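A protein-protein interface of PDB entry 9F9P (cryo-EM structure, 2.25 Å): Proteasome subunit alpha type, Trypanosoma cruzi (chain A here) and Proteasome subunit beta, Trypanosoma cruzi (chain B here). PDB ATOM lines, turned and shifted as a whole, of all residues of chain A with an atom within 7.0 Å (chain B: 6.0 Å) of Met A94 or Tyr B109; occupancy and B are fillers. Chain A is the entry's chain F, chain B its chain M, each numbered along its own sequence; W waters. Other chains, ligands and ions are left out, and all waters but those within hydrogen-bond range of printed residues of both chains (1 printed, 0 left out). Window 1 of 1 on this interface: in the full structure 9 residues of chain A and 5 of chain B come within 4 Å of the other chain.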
ATOM      1  N   GLU A  62       3.448   0.429 -15.605  1.00  0.00           N
ATOM      2  CA  GLU A  62       4.649  -0.141 -14.997  1.00  0.00           C
ATOM      3  C   GLU A  62       5.376  -1.081 -15.964  1.00  0.00           C
ATOM      4  O   GLU A  62       4.817  -2.083 -16.410  1.00  0.00           O
ATOM      5  CB  GLU A  62       4.248  -0.931 -13.743  1.00  0.00           C
ATOM      6  CG  GLU A  62       5.329  -1.014 -12.667  1.00  0.00           C
ATOM      7  CD  GLU A  62       5.113  -2.093 -11.611  1.00  0.00           C
ATOM      8  OE1 GLU A  62       3.950  -2.286 -11.185  1.00  0.00           O
ATOM      9  OE2 GLU A  62       6.110  -2.735 -11.202  1.00  0.00           O
ATOM     10  N   PHE A  65      10.822  -3.677 -13.115  1.00  0.00           N
ATOM     11  CA  PHE A  65      10.607  -4.418 -11.892  1.00  0.00           C
ATOM     12  C   PHE A  65      11.923  -4.861 -11.273  1.00  0.00           C
ATOM     13  O   PHE A  65      12.731  -5.465 -11.948  1.00  0.00           O
ATOM     14  CB  PHE A  65       9.894  -5.728 -12.173  1.00  0.00           C
ATOM     15  CG  PHE A  65       8.509  -5.621 -12.734  1.00  0.00           C
ATOM     16  CD1 PHE A  65       7.415  -6.029 -11.979  1.00  0.00           C
ATOM     17  CD2 PHE A  65       8.297  -5.212 -14.039  1.00  0.00           C
ATOM     18  CE1 PHE A  65       6.127  -5.967 -12.498  1.00  0.00           C
ATOM     19  CE2 PHE A  65       7.008  -5.138 -14.555  1.00  0.00           C
ATOM     20  CZ  PHE A  65       5.928  -5.520 -13.787  1.00  0.00           C
ATOM     21  N   LYS A  66      12.092  -4.652  -9.970  1.00  0.00           N
ATOM     22  CA  LYS A  66      13.210  -5.170  -9.200  1.00  0.00           C
ATOM     23  C   LYS A  66      13.041  -6.664  -8.899  1.00  0.00           C
ATOM     24  O   LYS A  66      11.962  -7.095  -8.520  1.00  0.00           O
ATOM     25  CB  LYS A  66      13.243  -4.353  -7.915  1.00  0.00           C
ATOM     26  CG  LYS A  66      14.366  -4.647  -6.928  1.00  0.00           C
ATOM     27  CD  LYS A  66      14.554  -3.514  -5.916  1.00  0.00           C
ATOM     28  CE  LYS A  66      15.465  -3.848  -4.749  1.00  0.00           C
ATOM     29  NZ  LYS A  66      14.985  -5.076  -4.060  1.00  0.00           N
ATOM     30  N   LEU A  67      14.083  -7.478  -9.068  1.00  0.00           N
ATOM     31  CA  LEU A  67      13.911  -8.891  -8.774  1.00  0.00           C
ATOM     32  C   LEU A  67      14.686  -9.333  -7.535  1.00  0.00           C
ATOM     33  O   LEU A  67      14.382 -10.372  -6.989  1.00  0.00           O
ATOM     34  CB  LEU A  67      14.257  -9.770  -9.983  1.00  0.00           C
ATOM     35  CG  LEU A  67      13.582  -9.407 -11.306  1.00  0.00           C
ATOM     36  CD1 LEU A  67      14.213 -10.145 -12.474  1.00  0.00           C
ATOM     37  CD2 LEU A  67      12.093  -9.722 -11.301  1.00  0.00           C
ATOM     38  N   ASP A  68      15.696  -8.588  -7.112  1.00  0.00           N
ATOM     39  CA  ASP A  68      16.474  -8.862  -5.908  1.00  0.00           C
ATOM     40  C   ASP A  68      17.407  -7.667  -5.812  1.00  0.00           C
ATOM     41  O   ASP A  68      17.369  -6.819  -6.688  1.00  0.00           O
ATOM     42  CB  ASP A  68      17.209 -10.217  -5.983  1.00  0.00           C
ATOM     43  CG  ASP A  68      17.584 -10.886  -4.646  1.00  0.00           C
ATOM     44  OD1 ASP A  68      18.703 -11.439  -4.556  1.00  0.00           O
ATOM     45  OD2 ASP A  68      16.743 -10.916  -3.687  1.00  0.00           O
ATOM     46  N   ASP A  69      18.304  -7.629  -4.822  1.00  0.00           N
ATOM     47  CA  ASP A  69      19.184  -6.477  -4.645  1.00  0.00           C
ATOM     48  C   ASP A  69      20.105  -6.268  -5.839  1.00  0.00           C
ATOM     49  O   ASP A  69      20.521  -5.158  -6.110  1.00  0.00           O
ATOM     50  CB  ASP A  69      20.022  -6.612  -3.369  1.00  0.00           C
ATOM     51  CG  ASP A  69      19.186  -6.810  -2.095  1.00  0.00           C
ATOM     52  OD1 ASP A  69      18.177  -6.061  -1.904  1.00  0.00           O
ATOM     53  OD2 ASP A  69      19.543  -7.711  -1.283  1.00  0.00           O
ATOM     54  N   VAL A  71      19.634  -7.388  -9.161  1.00  0.00           N
ATOM     55  CA  VAL A  71      19.075  -7.720 -10.462  1.00  0.00           C
ATOM     56  C   VAL A  71      17.663  -7.189 -10.651  1.00  0.00           C
ATOM     57  O   VAL A  71      16.874  -7.199  -9.733  1.00  0.00           O
ATOM     58  CB  VAL A  71      19.134  -9.241 -10.699  1.00  0.00           C
ATOM     59  CG1 VAL A  71      18.473 -10.047  -9.616  1.00  0.00           C
ATOM     60  CG2 VAL A  71      18.509  -9.653 -12.014  1.00  0.00           C
ATOM     61  N   ALA A  86       8.078 -12.307 -13.094  1.00  0.00           N
ATOM     62  CA  ALA A  86       8.641 -11.577 -11.957  1.00  0.00           C
ATOM     63  C   ALA A  86       8.426 -12.307 -10.639  1.00  0.00           C
ATOM     64  O   ALA A  86       9.374 -12.456  -9.896  1.00  0.00           O
ATOM     65  CB  ALA A  86       8.087 -10.214 -11.872  1.00  0.00           C
ATOM     66  N   VAL A  89      10.924 -15.429 -10.577  1.00  0.00           N
ATOM     67  CA  VAL A  89      12.327 -15.118 -10.388  1.00  0.00           C
ATOM     68  C   VAL A  89      12.580 -14.569  -8.991  1.00  0.00           C
ATOM     69  O   VAL A  89      13.624 -14.836  -8.425  1.00  0.00           O
ATOM     70  CB  VAL A  89      12.830 -14.111 -11.434  1.00  0.00           C
ATOM     71  CG1 VAL A  89      14.271 -13.653 -11.183  1.00  0.00           C
ATOM     72  CG2 VAL A  89      12.739 -14.703 -12.832  1.00  0.00           C
ATOM     73  N   ARG A  90      11.685 -13.722  -8.475  1.00  0.00           N
ATOM     74  CA  ARG A  90      11.792 -13.238  -7.115  1.00  0.00           C
ATOM     75  C   ARG A  90      11.915 -14.418  -6.153  1.00  0.00           C
ATOM     76  O   ARG A  90      12.799 -14.452  -5.314  1.00  0.00           O
ATOM     77  CB  ARG A  90      10.593 -12.351  -6.773  1.00  0.00           C
ATOM     78  CG  ARG A  90      10.761 -10.927  -7.298  1.00  0.00           C
ATOM     79  CD  ARG A  90       9.421 -10.225  -7.425  1.00  0.00           C
ATOM     80  NE  ARG A  90       9.621  -8.854  -7.796  1.00  0.00           N
ATOM     81  CZ  ARG A  90       8.633  -7.988  -7.977  1.00  0.00           C
ATOM     82  NH1 ARG A  90       7.378  -8.379  -7.821  1.00  0.00           N
ATOM     83  NH2 ARG A  90       8.954  -6.740  -8.296  1.00  0.00           N
ATOM     84  N   THR A  91      11.005 -15.378  -6.294  1.00  0.00           N
ATOM     85  CA  THR A  91      10.942 -16.498  -5.377  1.00  0.00           C
ATOM     86  C   THR A  91      12.221 -17.309  -5.414  1.00  0.00           C
ATOM     87  O   THR A  91      12.693 -17.702  -4.358  1.00  0.00           O
ATOM     88  CB  THR A  91       9.749 -17.389  -5.701  1.00  0.00           C
ATOM     89  OG1 THR A  91       8.558 -16.619  -5.504  1.00  0.00           O
ATOM     90  CG2 THR A  91       9.720 -18.655  -4.878  1.00  0.00           C
ATOM     91  N   GLU A  92      12.770 -17.538  -6.612  1.00  0.00           N
ATOM     92  CA  GLU A  92      14.026 -18.249  -6.832  1.00  0.00           C
ATOM     93  C   GLU A  92      15.230 -17.559  -6.192  1.00  0.00           C
ATOM     94  O   GLU A  92      16.117 -18.236  -5.673  1.00  0.00           O
ATOM     95  CB  GLU A  92      14.319 -18.309  -8.333  1.00  0.00           C
ATOM     96  CG  GLU A  92      14.228 -19.693  -8.939  1.00  0.00           C
ATOM     97  CD  GLU A  92      13.127 -20.663  -8.530  1.00  0.00           C
ATOM     98  OE1 GLU A  92      13.362 -21.894  -8.682  1.00  0.00           O
ATOM     99  OE2 GLU A  92      12.013 -20.208  -8.108  1.00  0.00           O
ATOM    100  N   CYS A  93      15.327 -16.245  -6.337  1.00  0.00           N
ATOM    101  CA  CYS A  93      16.392 -15.488  -5.722  1.00  0.00           C
ATOM    102  C   CYS A  93      16.282 -15.473  -4.199  1.00  0.00           C
ATOM    103  O   CYS A  93      17.312 -15.497  -3.541  1.00  0.00           O
ATOM    104  CB  CYS A  93      16.399 -14.047  -6.199  1.00  0.00           C
ATOM    105  SG  CYS A  93      16.922 -13.864  -7.924  1.00  0.00           S
ATOM    106  N   MET A  94      15.070 -15.443  -3.641  1.00  0.00           N
ATOM    107  CA  MET A  94      14.919 -15.510  -2.210  1.00  0.00           C
ATOM    108  C   MET A  94      15.374 -16.875  -1.679  1.00  0.00           C
ATOM    109  O   MET A  94      16.107 -16.926  -0.697  1.00  0.00           O
ATOM    110  CB  MET A  94      13.479 -15.256  -1.769  1.00  0.00           C
ATOM    111  CG  MET A  94      13.114 -13.782  -1.733  1.00  0.00           C
ATOM    112  SD  MET A  94      11.369 -13.518  -1.277  1.00  0.00           S
ATOM    113  CE  MET A  94      11.054 -11.974  -2.111  1.00  0.00           C
ATOM    114  N   ASN A  95      14.958 -17.970  -2.296  1.00  0.00           N
ATOM    115  CA  ASN A  95      15.469 -19.256  -1.879  1.00  0.00           C
ATOM    116  C   ASN A  95      16.998 -19.372  -1.984  1.00  0.00           C
ATOM    117  O   ASN A  95      17.628 -19.905  -1.093  1.00  0.00           O
ATOM    118  CB  ASN A  95      14.923 -20.412  -2.697  1.00  0.00           C
ATOM    119  CG  ASN A  95      13.443 -20.597  -2.554  1.00  0.00           C
ATOM    120  OD1 ASN A  95      12.829 -20.138  -1.601  1.00  0.00           O
ATOM    121  ND2 ASN A  95      12.836 -21.244  -3.543  1.00  0.00           N
ATOM    122  N   TYR A  96      17.601 -18.907  -3.057  1.00  0.00           N
ATOM    123  CA  TYR A  96      19.028 -19.008  -3.170  1.00  0.00           C
ATOM    124  C   TYR A  96      19.737 -18.310  -2.000  1.00  0.00           C
ATOM    125  O   TYR A  96      20.680 -18.861  -1.434  1.00  0.00           O
ATOM    126  CB  TYR A  96      19.546 -18.457  -4.497  1.00  0.00           C
ATOM    127  CG  TYR A  96      20.990 -18.809  -4.784  1.00  0.00           C
ATOM    128  CD1 TYR A  96      21.313 -19.980  -5.443  1.00  0.00           C
ATOM    129  CD2 TYR A  96      22.026 -18.014  -4.318  1.00  0.00           C
ATOM    130  CE1 TYR A  96      22.638 -20.363  -5.644  1.00  0.00           C
ATOM    131  CE2 TYR A  96      23.363 -18.358  -4.538  1.00  0.00           C
ATOM    132  CZ  TYR A  96      23.667 -19.555  -5.185  1.00  0.00           C
ATOM    133  OH  TYR A  96      24.984 -19.929  -5.397  1.00  0.00           O
ATOM    134  N   ARG A  97      19.289 -17.121  -1.635  1.00  0.00           N
ATOM    135  CA  ARG A  97      19.931 -16.374  -0.568  1.00  0.00           C
ATOM    136  C   ARG A  97      19.688 -17.042   0.801  1.00  0.00           C
ATOM    137  O   ARG A  97      20.573 -17.108   1.633  1.00  0.00           O
ATOM    138  CB  ARG A  97      19.466 -14.915  -0.594  1.00  0.00           C
ATOM    139  CG  ARG A  97      20.411 -14.011   0.184  1.00  0.00           C
ATOM    140  CD  ARG A  97      20.020 -12.549   0.323  1.00  0.00           C
ATOM    141  NE  ARG A  97      19.920 -11.918  -0.971  1.00  0.00           N
ATOM    142  CZ  ARG A  97      20.970 -11.449  -1.617  1.00  0.00           C
ATOM    143  NH1 ARG A  97      22.166 -11.493  -1.025  1.00  0.00           N
ATOM    144  NH2 ARG A  97      20.823 -10.974  -2.846  1.00  0.00           N
ATOM    145  N   TYR A  98      18.512 -17.595   1.018  1.00  0.00           N
ATOM    146  CA  TYR A  98      18.260 -18.341   2.229  1.00  0.00           C
ATOM    147  C   TYR A  98      19.298 -19.464   2.386  1.00  0.00           C
ATOM    148  O   TYR A  98      19.926 -19.596   3.440  1.00  0.00           O
ATOM    149  CB  TYR A  98      16.835 -18.867   2.233  1.00  0.00           C
ATOM    150  CG  TYR A  98      16.495 -19.756   3.388  1.00  0.00           C
ATOM    151  CD1 TYR A  98      16.297 -19.234   4.655  1.00  0.00           C
ATOM    152  CD2 TYR A  98      16.370 -21.144   3.223  1.00  0.00           C
ATOM    153  CE1 TYR A  98      15.959 -20.066   5.721  1.00  0.00           C
ATOM    154  CE2 TYR A  98      16.011 -21.992   4.279  1.00  0.00           C
ATOM    155  CZ  TYR A  98      15.789 -21.436   5.531  1.00  0.00           C
ATOM    156  OH  TYR A  98      15.515 -22.215   6.613  1.00  0.00           O
ATOM    157  N   MET A  99      19.523 -20.243   1.340  1.00  0.00           N
ATOM    158  CA  MET A  99      20.379 -21.409   1.441  1.00  0.00           C
ATOM    159  C   MET A  99      21.850 -21.049   1.382  1.00  0.00           C
ATOM    160  O   MET A  99      22.609 -21.796   1.937  1.00  0.00           O
ATOM    161  CB  MET A  99      20.087 -22.404   0.328  1.00  0.00           C
ATOM    162  CG  MET A  99      18.697 -22.987   0.372  1.00  0.00           C
ATOM    163  SD  MET A  99      18.343 -24.052   1.825  1.00  0.00           S
ATOM    164  CE  MET A  99      19.473 -25.418   1.579  1.00  0.00           C
ATOM    165  N   ASN A 104      22.138 -14.862  -5.975  1.00  0.00           N
ATOM    166  CA  ASN A 104      21.897 -15.883  -7.030  1.00  0.00           C
ATOM    167  C   ASN A 104      22.668 -15.507  -8.299  1.00  0.00           C
ATOM    168  O   ASN A 104      22.474 -14.401  -8.802  1.00  0.00           O
ATOM    169  CB  ASN A 104      20.385 -15.980  -7.313  1.00  0.00           C
ATOM    170  CG  ASN A 104      19.899 -17.177  -8.085  1.00  0.00           C
ATOM    171  OD1 ASN A 104      18.711 -17.408  -8.277  1.00  0.00           O
ATOM    172  ND2 ASN A 104      20.805 -17.988  -8.552  1.00  0.00           N
ATOM    173  N   TYR B 102      11.686 -12.135   4.635  1.00  0.00           N
ATOM    174  CA  TYR B 102      11.009 -12.459   3.388  1.00  0.00           C
ATOM    175  C   TYR B 102       9.566 -11.952   3.347  1.00  0.00           C
ATOM    176  O   TYR B 102       9.224 -11.394   2.316  1.00  0.00           O
ATOM    177  CB  TYR B 102      11.242 -13.936   3.031  1.00  0.00           C
ATOM    178  CG  TYR B 102      12.712 -14.116   2.699  1.00  0.00           C
ATOM    179  CD1 TYR B 102      13.342 -13.213   1.846  1.00  0.00           C
ATOM    180  CD2 TYR B 102      13.518 -15.060   3.335  1.00  0.00           C
ATOM    181  CE1 TYR B 102      14.700 -13.309   1.555  1.00  0.00           C
ATOM    182  CE2 TYR B 102      14.894 -15.130   3.103  1.00  0.00           C
ATOM    183  CZ  TYR B 102      15.484 -14.269   2.185  1.00  0.00           C
ATOM    184  OH  TYR B 102      16.819 -14.289   1.875  1.00  0.00           O
ATOM    185  N   ILE B 104       8.565  -9.251   4.710  1.00  0.00           N
ATOM    186  CA  ILE B 104       8.692  -7.813   4.573  1.00  0.00           C
ATOM    187  C   ILE B 104       9.087  -7.446   3.149  1.00  0.00           C
ATOM    188  O   ILE B 104       8.692  -6.405   2.657  1.00  0.00           O
ATOM    189  CB  ILE B 104       9.667  -7.264   5.642  1.00  0.00           C
ATOM    190  CG1 ILE B 104       9.065  -7.367   7.048  1.00  0.00           C
ATOM    191  CG2 ILE B 104      10.098  -5.866   5.377  1.00  0.00           C
ATOM    192  CD1 ILE B 104      10.061  -7.157   8.193  1.00  0.00           C
ATOM    193  N   GLN B 105       9.863  -8.287   2.493  1.00  0.00           N
ATOM    194  CA  GLN B 105      10.221  -8.108   1.098  1.00  0.00           C
ATOM    195  C   GLN B 105       9.003  -8.244   0.186  1.00  0.00           C
ATOM    196  O   GLN B 105       8.778  -7.366  -0.620  1.00  0.00           O
ATOM    197  CB  GLN B 105      11.376  -9.067   0.800  1.00  0.00           C
ATOM    198  CG  GLN B 105      12.156  -8.752  -0.447  1.00  0.00           C
ATOM    199  CD  GLN B 105      12.454  -7.271  -0.564  1.00  0.00           C
ATOM    200  OE1 GLN B 105      13.329  -6.741   0.126  1.00  0.00           O
ATOM    201  NE2 GLN B 105      11.722  -6.584  -1.444  1.00  0.00           N
ATOM    202  N   TRP B 106       8.149  -9.254   0.405  1.00  0.00           N
ATOM    203  CA  TRP B 106       6.898  -9.379  -0.314  1.00  0.00           C
ATOM    204  C   TRP B 106       6.007  -8.157  -0.092  1.00  0.00           C
ATOM    205  O   TRP B 106       5.478  -7.617  -1.052  1.00  0.00           O
ATOM    206  CB  TRP B 106       6.167 -10.688  -0.013  1.00  0.00           C
ATOM    207  CG  TRP B 106       6.752 -11.901  -0.680  1.00  0.00           C
ATOM    208  CD1 TRP B 106       7.364 -12.962  -0.070  1.00  0.00           C
ATOM    209  CD2 TRP B 106       6.909 -12.150  -2.090  1.00  0.00           C
ATOM    210  NE1 TRP B 106       7.904 -13.827  -0.988  1.00  0.00           N
ATOM    211  CE2 TRP B 106       7.624 -13.363  -2.235  1.00  0.00           C
ATOM    212  CE3 TRP B 106       6.563 -11.439  -3.242  1.00  0.00           C
ATOM    213  CZ2 TRP B 106       7.907 -13.931  -3.467  1.00  0.00           C
ATOM    214  CZ3 TRP B 106       6.843 -12.006  -4.472  1.00  0.00           C
ATOM    215  CH2 TRP B 106       7.475 -13.245  -4.576  1.00  0.00           C
ATOM    216  N   TYR B 107       5.863  -7.646   1.133  1.00  0.00           N
ATOM    217  CA  TYR B 107       5.113  -6.425   1.356  1.00  0.00           C
ATOM    218  C   TYR B 107       5.627  -5.292   0.486  1.00  0.00           C
ATOM    219  O   TYR B 107       4.838  -4.592  -0.093  1.00  0.00           O
ATOM    220  CB  TYR B 107       5.114  -6.046   2.849  1.00  0.00           C
ATOM    221  CG  TYR B 107       4.380  -4.792   3.279  1.00  0.00           C
ATOM    222  CD1 TYR B 107       4.838  -3.527   2.972  1.00  0.00           C
ATOM    223  CD2 TYR B 107       3.199  -4.891   3.973  1.00  0.00           C
ATOM    224  CE1 TYR B 107       4.154  -2.377   3.349  1.00  0.00           C
ATOM    225  CE2 TYR B 107       2.513  -3.770   4.393  1.00  0.00           C
ATOM    226  CZ  TYR B 107       2.986  -2.509   4.083  1.00  0.00           C
ATOM    227  OH  TYR B 107       2.280  -1.439   4.525  1.00  0.00           O
ATOM    228  N   GLN B 108       6.904  -5.049   0.381  1.00  0.00           N
ATOM    229  CA  GLN B 108       7.338  -3.992  -0.517  1.00  0.00           C
ATOM    230  C   GLN B 108       6.979  -4.270  -1.986  1.00  0.00           C
ATOM    231  O   GLN B 108       6.636  -3.361  -2.714  1.00  0.00           O
ATOM    232  CB  GLN B 108       8.849  -3.842  -0.546  1.00  0.00           C
ATOM    233  CG  GLN B 108       9.468  -3.402   0.760  1.00  0.00           C
ATOM    234  CD  GLN B 108      10.938  -3.086   0.558  1.00  0.00           C
ATOM    235  OE1 GLN B 108      11.817  -3.859   0.927  1.00  0.00           O
ATOM    236  NE2 GLN B 108      11.217  -1.941  -0.042  1.00  0.00           N
ATOM    237  N   TYR B 109       7.111  -5.495  -2.482  1.00  0.00           N
ATOM    238  CA  TYR B 109       6.784  -5.759  -3.878  1.00  0.00           C
ATOM    239  C   TYR B 109       5.299  -5.547  -4.185  1.00  0.00           C
ATOM    240  O   TYR B 109       4.983  -5.173  -5.299  1.00  0.00           O
ATOM    241  CB  TYR B 109       7.177  -7.181  -4.273  1.00  0.00           C
ATOM    242  CG  TYR B 109       8.659  -7.443  -4.322  1.00  0.00           C
ATOM    243  CD1 TYR B 109       9.536  -6.496  -4.797  1.00  0.00           C
ATOM    244  CD2 TYR B 109       9.174  -8.682  -3.969  1.00  0.00           C
ATOM    245  CE1 TYR B 109      10.891  -6.746  -4.869  1.00  0.00           C
ATOM    246  CE2 TYR B 109      10.530  -8.964  -4.044  1.00  0.00           C
ATOM    247  CZ  TYR B 109      11.386  -7.989  -4.525  1.00  0.00           C
ATOM    248  OH  TYR B 109      12.747  -8.175  -4.572  1.00  0.00           O
ATOM    249  N   ASN B 110       4.407  -5.823  -3.227  1.00  0.00           N
ATOM    250  CA  ASN B 110       2.976  -5.612  -3.350  1.00  0.00           C
ATOM    251  C   ASN B 110       2.510  -4.223  -2.916  1.00  0.00           C
ATOM    252  O   ASN B 110       1.330  -3.933  -3.015  1.00  0.00           O
ATOM    253  CB  ASN B 110       2.192  -6.605  -2.503  1.00  0.00           C
ATOM    254  CG  ASN B 110       2.529  -8.021  -2.900  1.00  0.00           C
ATOM    255  OD1 ASN B 110       2.861  -8.261  -4.061  1.00  0.00           O
ATOM    256  ND2 ASN B 110       2.518  -8.952  -1.950  1.00  0.00           N
ATOM    257  N   ASN B 111       3.392  -3.347  -2.450  1.00  0.00           N
ATOM    258  CA  ASN B 111       2.945  -2.026  -2.024  1.00  0.00           C
ATOM    259  C   ASN B 111       3.827  -0.940  -2.610  1.00  0.00           C
ATOM    260  O   ASN B 111       4.103   0.057  -1.970  1.00  0.00           O
ATOM    261  CB  ASN B 111       2.905  -1.862  -0.499  1.00  0.00           C
ATOM    262  CG  ASN B 111       1.843  -2.704   0.174  1.00  0.00           C
ATOM    263  OD1 ASN B 111       0.759  -2.214   0.457  1.00  0.00           O
ATOM    264  ND2 ASN B 111       2.118  -3.961   0.478  1.00  0.00           N
ATOM    265  N   GLY B 112       4.246  -1.044  -3.845  1.00  0.00           N
ATOM    266  CA  GLY B 112       4.822   0.147  -4.452  1.00  0.00           C
ATOM    267  C   GLY B 112       6.208   0.497  -3.909  1.00  0.00           C
ATOM    268  O   GLY B 112       6.653   1.630  -4.050  1.00  0.00           O
ATOM    269  N   GLY B 113       6.904  -0.475  -3.309  1.00  0.00           N
ATOM    270  CA  GLY B 113       8.257  -0.250  -2.840  1.00  0.00           C
ATOM    271  C   GLY B 113       8.352   0.218  -1.390  1.00  0.00           C
ATOM    272  O   GLY B 113       9.463   0.260  -0.863  1.00  0.00           O
HETATM  273  O   HOH W   1       5.926  -5.579  -7.883  1.00  0.00           O
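The indole nitrogen (NE1) of Trp B106 lies within hydrogen-bond range of the side-chain sulfur (SD) of Met A94, 3.5 Å away.
OE1 of Gln B105 sits close to OE1 of Gln B108 (3.4 Å). O of Trp B106 is in hydrogen-bond range of ND2 of Asn B110 (3.4 Å). NZ of Lys A66 is in salt-bridge range of OD1 of Asp A69 (3.98 Å). The backbone carbonyl oxygen of Lys A66 sits at hydrogen-bond distance from the guanidinium group of Arg A90. The side-chain carboxylate of Asp A68 lies within salt-bridge range of the guanidinium group of Arg A97. OD2 of Asp A69 lies within salt-bridge range of NH2 of Arg A97 (3.8 Å).
O of Lys A66 touches CE1 of Tyr B109 (3.8 Å). OH of Tyr B109 touches O of Leu A67 (3.7 Å). OH of Tyr B109 touches N of Asp A68 (3.9 Å). Trp B106 touches Arg A90. NH2 of Arg A90 touches CD1 of Tyr B109, at 3.6 Å. Thr A91 touches Trp B106 (OG1 to CZ2, 3.4 Å). Tyr B102 touches Met A94 (CD1 to CG, 3.6 Å). Met A94 touches Gln B105 (CE to CG, 3.8 Å). Tyr B109 touches Met A94 (CE2 to CE, 3.6 Å). Arg A97 touches Tyr B102.
Of chain B, only Tyr B102 (3.6 Å), Gln B105 (3.8 Å), Trp B106 (3.5 Å) and Tyr B109 (3.6 Å) come within 4 Å of Met A94. Of the printed residues of chain A, Gln B105 touches Met A94. Of the printed residues of chain B, Lys A66 touches Tyr B109. Printed residues of chain B within 4 Å of Arg A90: Trp B106 (3.9 Å) and Tyr B109 (3.6 Å). Of the printed residues of chain A, Tyr B102 touches Met A94 (3.6 Å), Arg A97 (3.7 Å) and Tyr A98 (3.8 Å). The nearest printed residue of chain B that does not touch Met A94 is Ile B104 (7.2 Å). The nearest printed residue of chain B that does not touch Arg A90 is Asn B110 (5.9 Å).
Printed residues of chain B that touch a printed residue of chain A: Tyr B102, Gln B105, Trp B106 and Tyr B109. Hydrophobic or aromatic side chains of chain B that line the printed part of chain A: Tyr B102, Trp B106 and Tyr B109. Hydrophobic or aromatic side chains of chain A within 4 Å of the printed part of chain B: Met A94. Among the printed residues, 12 pairs touch across the chains. Among the printed residues, no Asp or Glu carboxylate lies within 4 Å of a Lys or Arg side-chain nitrogen of the other chain.
Water W1 lies within hydrogen-bond range of the backbone carbonyl oxygen of Tyr B109 (2.8 Å) and the guanidinium group of Arg A90 (3.2 Å).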
